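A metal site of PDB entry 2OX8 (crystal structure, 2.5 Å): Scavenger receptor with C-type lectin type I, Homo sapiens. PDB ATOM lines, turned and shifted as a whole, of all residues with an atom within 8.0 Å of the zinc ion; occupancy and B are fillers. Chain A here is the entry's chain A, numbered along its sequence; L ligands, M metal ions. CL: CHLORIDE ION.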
ATOM      1  N   PHE A  12     -10.581 -13.778 -17.060  1.00  0.00           N
ATOM      2  CA  PHE A  12      -9.892 -12.665 -17.690  1.00  0.00           C
ATOM      3  C   PHE A  12     -10.369 -12.687 -19.126  1.00  0.00           C
ATOM      4  O   PHE A  12     -10.202 -13.679 -19.833  1.00  0.00           O
ATOM      5  CB  PHE A  12      -8.371 -12.876 -17.672  1.00  0.00           C
ATOM      6  CG  PHE A  12      -7.611 -11.820 -18.447  1.00  0.00           C
ATOM      7  CD1 PHE A  12      -7.395 -10.559 -17.909  1.00  0.00           C
ATOM      8  CD2 PHE A  12      -7.139 -12.098 -19.730  1.00  0.00           C
ATOM      9  CE1 PHE A  12      -6.717  -9.569 -18.626  1.00  0.00           C
ATOM     10  CE2 PHE A  12      -6.466 -11.116 -20.457  1.00  0.00           C
ATOM     11  CZ  PHE A  12      -6.257  -9.850 -19.901  1.00  0.00           C
ATOM     12  N   ASP A  14     -12.527 -13.529 -21.917  1.00  0.00           N
ATOM     13  CA  ASP A  14     -13.593 -14.524 -22.081  1.00  0.00           C
ATOM     14  C   ASP A  14     -13.088 -15.920 -21.734  1.00  0.00           C
ATOM     15  O   ASP A  14     -13.680 -16.923 -22.128  1.00  0.00           O
ATOM     16  CB  ASP A  14     -14.110 -14.509 -23.520  1.00  0.00           C
ATOM     17  CG  ASP A  14     -13.090 -15.001 -24.526  1.00  0.00           C
ATOM     18  OD1 ASP A  14     -11.868 -14.889 -24.269  1.00  0.00           O
ATOM     19  OD2 ASP A  14     -13.505 -15.490 -25.599  1.00  0.00           O
ATOM     20  N   LYS A  15     -12.006 -15.963 -20.972  1.00  0.00           N
ATOM     21  CA  LYS A  15     -11.395 -17.233 -20.627  1.00  0.00           C
ATOM     22  C   LYS A  15     -11.279 -17.525 -19.132  1.00  0.00           C
ATOM     23  O   LYS A  15     -11.039 -16.621 -18.300  1.00  0.00           O
ATOM     24  CB  LYS A  15     -10.000 -17.300 -21.236  1.00  0.00           C
ATOM     25  CG  LYS A  15      -9.960 -16.919 -22.693  1.00  0.00           C
ATOM     26  CD  LYS A  15      -8.536 -16.761 -23.173  1.00  0.00           C
ATOM     27  CE  LYS A  15      -8.492 -16.679 -24.670  1.00  0.00           C
ATOM     28  NZ  LYS A  15      -9.262 -15.506 -25.085  1.00  0.00           N
ATOM     29  N   TYR A  17      -9.254 -19.568 -16.288  1.00  0.00           N
ATOM     30  CA  TYR A  17      -7.926 -20.109 -16.017  1.00  0.00           C
ATOM     31  C   TYR A  17      -7.898 -20.936 -14.730  1.00  0.00           C
ATOM     32  O   TYR A  17      -8.589 -20.652 -13.767  1.00  0.00           O
ATOM     33  CB  TYR A  17      -6.912 -18.970 -15.914  1.00  0.00           C
ATOM     34  CG  TYR A  17      -6.750 -18.150 -17.165  1.00  0.00           C
ATOM     35  CD1 TYR A  17      -7.724 -17.258 -17.565  1.00  0.00           C
ATOM     36  CD2 TYR A  17      -5.623 -18.300 -17.974  1.00  0.00           C
ATOM     37  CE1 TYR A  17      -7.583 -16.521 -18.743  1.00  0.00           C
ATOM     38  CE2 TYR A  17      -5.477 -17.586 -19.154  1.00  0.00           C
ATOM     39  CZ  TYR A  17      -6.460 -16.686 -19.527  1.00  0.00           C
ATOM     40  OH  TYR A  17      -6.304 -15.938 -20.681  1.00  0.00           O
ATOM     41  N   HIS A  39      -6.781 -26.763 -21.949  1.00  0.00           N
ATOM     42  CA  HIS A  39      -5.449 -27.126 -22.358  1.00  0.00           C
ATOM     43  C   HIS A  39      -4.486 -26.209 -21.643  1.00  0.00           C
ATOM     44  O   HIS A  39      -4.887 -25.136 -21.196  1.00  0.00           O
ATOM     45  CB  HIS A  39      -5.293 -26.890 -23.862  1.00  0.00           C
ATOM     46  CG  HIS A  39      -5.782 -25.551 -24.308  1.00  0.00           C
ATOM     47  ND1 HIS A  39      -5.117 -24.379 -24.017  1.00  0.00           N
ATOM     48  CD2 HIS A  39      -6.915 -25.190 -24.964  1.00  0.00           C
ATOM     49  CE1 HIS A  39      -5.812 -23.348 -24.472  1.00  0.00           C
ATOM     50  NE2 HIS A  39      -6.906 -23.814 -25.050  1.00  0.00           N
ATOM     51  N   LEU A  40      -3.236 -26.644 -21.518  1.00  0.00           N
ATOM     52  CA  LEU A  40      -2.244 -25.820 -20.887  1.00  0.00           C
ATOM     53  C   LEU A  40      -2.373 -24.451 -21.592  1.00  0.00           C
ATOM     54  O   LEU A  40      -2.534 -24.354 -22.822  1.00  0.00           O
ATOM     55  CB  LEU A  40      -0.866 -26.465 -21.040  1.00  0.00           C
ATOM     56  CG  LEU A  40      -0.607 -27.647 -20.061  1.00  0.00           C
ATOM     57  CD1 LEU A  40       0.546 -28.510 -20.544  1.00  0.00           C
ATOM     58  CD2 LEU A  40      -0.322 -27.105 -18.652  1.00  0.00           C
ATOM     59  N   VAL A  41      -2.343 -23.404 -20.767  1.00  0.00           N
ATOM     60  CA  VAL A  41      -2.510 -22.027 -21.189  1.00  0.00           C
ATOM     61  C   VAL A  41      -1.659 -21.556 -22.393  1.00  0.00           C
ATOM     62  O   VAL A  41      -0.514 -21.973 -22.564  1.00  0.00           O
ATOM     63  CB  VAL A  41      -2.242 -21.099 -19.981  1.00  0.00           C
ATOM     64  CG1 VAL A  41      -0.778 -21.140 -19.605  1.00  0.00           C
ATOM     65  CG2 VAL A  41      -2.670 -19.698 -20.270  1.00  0.00           C
ATOM     66  N   PHE A  42      -2.261 -20.706 -23.224  1.00  0.00           N
ATOM     67  CA  PHE A  42      -1.587 -20.108 -24.385  1.00  0.00           C
ATOM     68  C   PHE A  42      -1.530 -18.635 -23.988  1.00  0.00           C
ATOM     69  O   PHE A  42      -2.522 -18.084 -23.498  1.00  0.00           O
ATOM     70  CB  PHE A  42      -2.418 -20.201 -25.668  1.00  0.00           C
ATOM     71  CG  PHE A  42      -2.648 -21.582 -26.163  1.00  0.00           C
ATOM     72  CD1 PHE A  42      -3.736 -21.856 -26.963  1.00  0.00           C
ATOM     73  CD2 PHE A  42      -1.797 -22.622 -25.805  1.00  0.00           C
ATOM     74  CE1 PHE A  42      -3.994 -23.159 -27.403  1.00  0.00           C
ATOM     75  CE2 PHE A  42      -2.041 -23.927 -26.240  1.00  0.00           C
ATOM     76  CZ  PHE A  42      -3.159 -24.196 -27.040  1.00  0.00           C
ATOM     77  N   ILE A  43      -0.379 -17.997 -24.170  1.00  0.00           N
ATOM     78  CA  ILE A  43      -0.254 -16.587 -23.830  1.00  0.00           C
ATOM     79  C   ILE A  43      -0.007 -15.808 -25.117  1.00  0.00           C
ATOM     80  O   ILE A  43       1.096 -15.832 -25.664  1.00  0.00           O
ATOM     81  CB  ILE A  43       0.886 -16.379 -22.828  1.00  0.00           C
ATOM     82  CG1 ILE A  43       0.545 -17.101 -21.536  1.00  0.00           C
ATOM     83  CG2 ILE A  43       1.120 -14.897 -22.593  1.00  0.00           C
ATOM     84  CD1 ILE A  43       1.718 -17.397 -20.666  1.00  0.00           C
ATOM     85  N   ASN A  44      -1.031 -15.119 -25.604  1.00  0.00           N
ATOM     86  CA  ASN A  44      -0.907 -14.413 -26.867  1.00  0.00           C
ATOM     87  C   ASN A  44      -0.882 -12.880 -26.907  1.00  0.00           C
ATOM     88  O   ASN A  44      -0.964 -12.297 -27.984  1.00  0.00           O
ATOM     89  CB  ASN A  44      -1.977 -14.920 -27.820  1.00  0.00           C
ATOM     90  CG  ASN A  44      -1.713 -16.331 -28.245  1.00  0.00           C
ATOM     91  OD1 ASN A  44      -0.663 -16.631 -28.815  1.00  0.00           O
ATOM     92  ND2 ASN A  44      -2.651 -17.228 -27.977  1.00  0.00           N
ATOM     93  N   THR A  45      -0.741 -12.244 -25.753  1.00  0.00           N
ATOM     94  CA  THR A  45      -0.695 -10.801 -25.715  1.00  0.00           C
ATOM     95  C   THR A  45      -0.017 -10.425 -24.428  1.00  0.00           C
ATOM     96  O   THR A  45      -0.053 -11.184 -23.471  1.00  0.00           O
ATOM     97  CB  THR A  45      -2.111 -10.184 -25.711  1.00  0.00           C
ATOM     98  OG1 THR A  45      -2.868 -10.746 -24.622  1.00  0.00           O
ATOM     99  CG2 THR A  45      -2.821 -10.464 -27.027  1.00  0.00           C
ATOM    100  N   GLU A  48      -2.414 -10.194 -21.429  1.00  0.00           N
ATOM    101  CA  GLU A  48      -2.747 -11.472 -20.824  1.00  0.00           C
ATOM    102  C   GLU A  48      -1.564 -11.868 -19.931  1.00  0.00           C
ATOM    103  O   GLU A  48      -1.745 -12.201 -18.768  1.00  0.00           O
ATOM    104  CB  GLU A  48      -3.017 -12.550 -21.888  1.00  0.00           C
ATOM    105  CG  GLU A  48      -3.432 -13.912 -21.330  1.00  0.00           C
ATOM    106  CD  GLU A  48      -3.646 -14.980 -22.400  1.00  0.00           C
ATOM    107  OE1 GLU A  48      -4.106 -16.099 -22.074  1.00  0.00           O
ATOM    108  OE2 GLU A  48      -3.356 -14.721 -23.568  1.00  0.00           O
ATOM    109  N   GLN A  49      -0.365 -11.801 -20.484  1.00  0.00           N
ATOM    110  CA  GLN A  49       0.851 -12.135 -19.740  1.00  0.00           C
ATOM    111  C   GLN A  49       0.958 -11.325 -18.442  1.00  0.00           C
ATOM    112  O   GLN A  49       1.355 -11.851 -17.418  1.00  0.00           O
ATOM    113  CB  GLN A  49       2.096 -11.916 -20.611  1.00  0.00           C
ATOM    114  CG  GLN A  49       3.426 -11.997 -19.894  1.00  0.00           C
ATOM    115  CD  GLN A  49       3.738 -13.381 -19.375  1.00  0.00           C
ATOM    116  OE1 GLN A  49       3.946 -14.316 -20.152  1.00  0.00           O
ATOM    117  NE2 GLN A  49       3.796 -13.522 -18.045  1.00  0.00           N
ATOM    118  N   TRP A  51      -1.524 -10.162 -16.715  1.00  0.00           N
ATOM    119  CA  TRP A  51      -2.601 -10.604 -15.829  1.00  0.00           C
ATOM    120  C   TRP A  51      -2.235 -11.913 -15.171  1.00  0.00           C
ATOM    121  O   TRP A  51      -2.406 -12.100 -13.973  1.00  0.00           O
ATOM    122  CB  TRP A  51      -3.894 -10.795 -16.604  1.00  0.00           C
ATOM    123  CG  TRP A  51      -4.998 -11.329 -15.755  1.00  0.00           C
ATOM    124  CD1 TRP A  51      -5.756 -10.613 -14.870  1.00  0.00           C
ATOM    125  CD2 TRP A  51      -5.462 -12.688 -15.666  1.00  0.00           C
ATOM    126  NE1 TRP A  51      -6.661 -11.440 -14.248  1.00  0.00           N
ATOM    127  CE2 TRP A  51      -6.506 -12.719 -14.707  1.00  0.00           C
ATOM    128  CE3 TRP A  51      -5.099 -13.882 -16.310  1.00  0.00           C
ATOM    129  CZ2 TRP A  51      -7.183 -13.904 -14.371  1.00  0.00           C
ATOM    130  CZ3 TRP A  51      -5.770 -15.058 -15.964  1.00  0.00           C
ATOM    131  CH2 TRP A  51      -6.804 -15.053 -15.001  1.00  0.00           C
ATOM    132  N   ILE A  52      -1.736 -12.843 -15.993  1.00  0.00           N
ATOM    133  CA  ILE A  52      -1.343 -14.146 -15.503  1.00  0.00           C
ATOM    134  C   ILE A  52      -0.351 -14.030 -14.358  1.00  0.00           C
ATOM    135  O   ILE A  52      -0.439 -14.757 -13.374  1.00  0.00           O
ATOM    136  CB  ILE A  52      -0.763 -14.985 -16.654  1.00  0.00           C
ATOM    137  CG1 ILE A  52      -1.912 -15.501 -17.522  1.00  0.00           C
ATOM    138  CG2 ILE A  52       0.071 -16.144 -16.123  1.00  0.00           C
ATOM    139  CD1 ILE A  52      -1.478 -16.266 -18.769  1.00  0.00           C
ATOM    140  N   TRP A  77       2.395 -23.374 -29.775  1.00  0.00           N
ATOM    141  CA  TRP A  77       1.397 -23.560 -28.742  1.00  0.00           C
ATOM    142  C   TRP A  77       0.703 -24.862 -29.135  1.00  0.00           C
ATOM    143  O   TRP A  77       0.665 -25.180 -30.329  1.00  0.00           O
ATOM    144  CB  TRP A  77       0.403 -22.415 -28.774  1.00  0.00           C
ATOM    145  CG  TRP A  77       0.992 -21.108 -28.385  1.00  0.00           C
ATOM    146  CD1 TRP A  77       1.143 -20.010 -29.186  1.00  0.00           C
ATOM    147  CD2 TRP A  77       1.453 -20.731 -27.086  1.00  0.00           C
ATOM    148  NE1 TRP A  77       1.670 -18.972 -28.450  1.00  0.00           N
ATOM    149  CE2 TRP A  77       1.874 -19.383 -27.164  1.00  0.00           C
ATOM    150  CE3 TRP A  77       1.557 -21.401 -25.854  1.00  0.00           C
ATOM    151  CZ2 TRP A  77       2.387 -18.695 -26.073  1.00  0.00           C
ATOM    152  CZ3 TRP A  77       2.073 -20.700 -24.766  1.00  0.00           C
ATOM    153  CH2 TRP A  77       2.483 -19.365 -24.877  1.00  0.00           C
ATOM    154  N   GLU A 129      -6.438 -23.526 -19.327  1.00  0.00           N
ATOM    155  CA  GLU A 129      -7.175 -22.437 -19.914  1.00  0.00           C
ATOM    156  C   GLU A 129      -8.256 -22.964 -20.865  1.00  0.00           C
ATOM    157  O   GLU A 129      -8.088 -24.040 -21.459  1.00  0.00           O
ATOM    158  CB  GLU A 129      -6.176 -21.548 -20.665  1.00  0.00           C
ATOM    159  CG  GLU A 129      -6.761 -20.419 -21.521  1.00  0.00           C
ATOM    160  CD  GLU A 129      -5.715 -19.769 -22.425  1.00  0.00           C
ATOM    161  OE1 GLU A 129      -5.094 -20.481 -23.226  1.00  0.00           O
ATOM    162  OE2 GLU A 129      -5.528 -18.535 -22.340  1.00  0.00           O
ATOM    163  N   LYS A 130      -9.350 -22.223 -20.974  1.00  0.00           N
ATOM    164  CA  LYS A 130     -10.431 -22.571 -21.891  1.00  0.00           C
ATOM    165  C   LYS A 130     -11.265 -21.320 -22.154  1.00  0.00           C
ATOM    166  O   LYS A 130     -11.569 -20.561 -21.235  1.00  0.00           O
ATOM    167  CB  LYS A 130     -11.308 -23.705 -21.353  1.00  0.00           C
ATOM    168  CG  LYS A 130     -11.969 -23.434 -20.013  1.00  0.00           C
ATOM    169  CD  LYS A 130     -12.849 -24.625 -19.623  1.00  0.00           C
ATOM    170  CE  LYS A 130     -13.193 -24.643 -18.140  1.00  0.00           C
ATOM    171  NZ  LYS A 130     -13.785 -25.971 -17.808  1.00  0.00           N
ATOM    172  N   ASP A 131     -11.605 -21.098 -23.418  1.00  0.00           N
ATOM    173  CA  ASP A 131     -12.383 -19.947 -23.840  1.00  0.00           C
ATOM    174  C   ASP A 131     -13.875 -20.308 -23.839  1.00  0.00           C
ATOM    175  O   ASP A 131     -14.289 -21.258 -24.486  1.00  0.00           O
ATOM    176  CB  ASP A 131     -11.893 -19.518 -25.245  1.00  0.00           C
ATOM    177  CG  ASP A 131     -12.800 -18.509 -25.910  1.00  0.00           C
ATOM    178  OD1 ASP A 131     -14.005 -18.787 -26.099  1.00  0.00           O
ATOM    179  OD2 ASP A 131     -12.322 -17.425 -26.274  1.00  0.00           O
HETATM  180 CL    CL L   1      -4.687 -17.076 -25.512  1.00  0.00          CL
HETATM  181 ZN    ZN M   1      -4.526 -17.445 -23.461  1.00  0.00          ZN
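Tyr 17 touches the zinc ion (OH to ZN, 3.6 Å). Within 4 Å of the zinc ion: Tyr 17, Phe 42, Glu 48 and Glu 129. The nearest printed residue that does not touch the zinc ion is Lys 15 (4.1 Å).
The zinc ion is bound by the side-chain carboxylate (OE2) of Glu 129, the side-chain carboxylate (OE1) of Glu 48, a chlorine (CL) of the ligand and the backbone carbonyl oxygen (O) of Phe 42. The zinc ion has four donor atoms within binding distance.
OH of Tyr 17 lies close to OE2 of Glu 129 (3.2 Å). The side-chain hydroxyl (OH) of Tyr 17 lies close to the side-chain carboxylate (OE1) of Glu 48, at 2.6 Å. OG1 of Thr 45 lies within hydrogen-bond range of N of Glu 48, at 3.3 Å. The backbone NH of Asn 44 lies within hydrogen-bond range of the side-chain carboxylate of Glu 48, 3.1 Å away. The backbone NH of Glu 129 lies within hydrogen-bond range of the backbone carbonyl oxygen of His 39.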
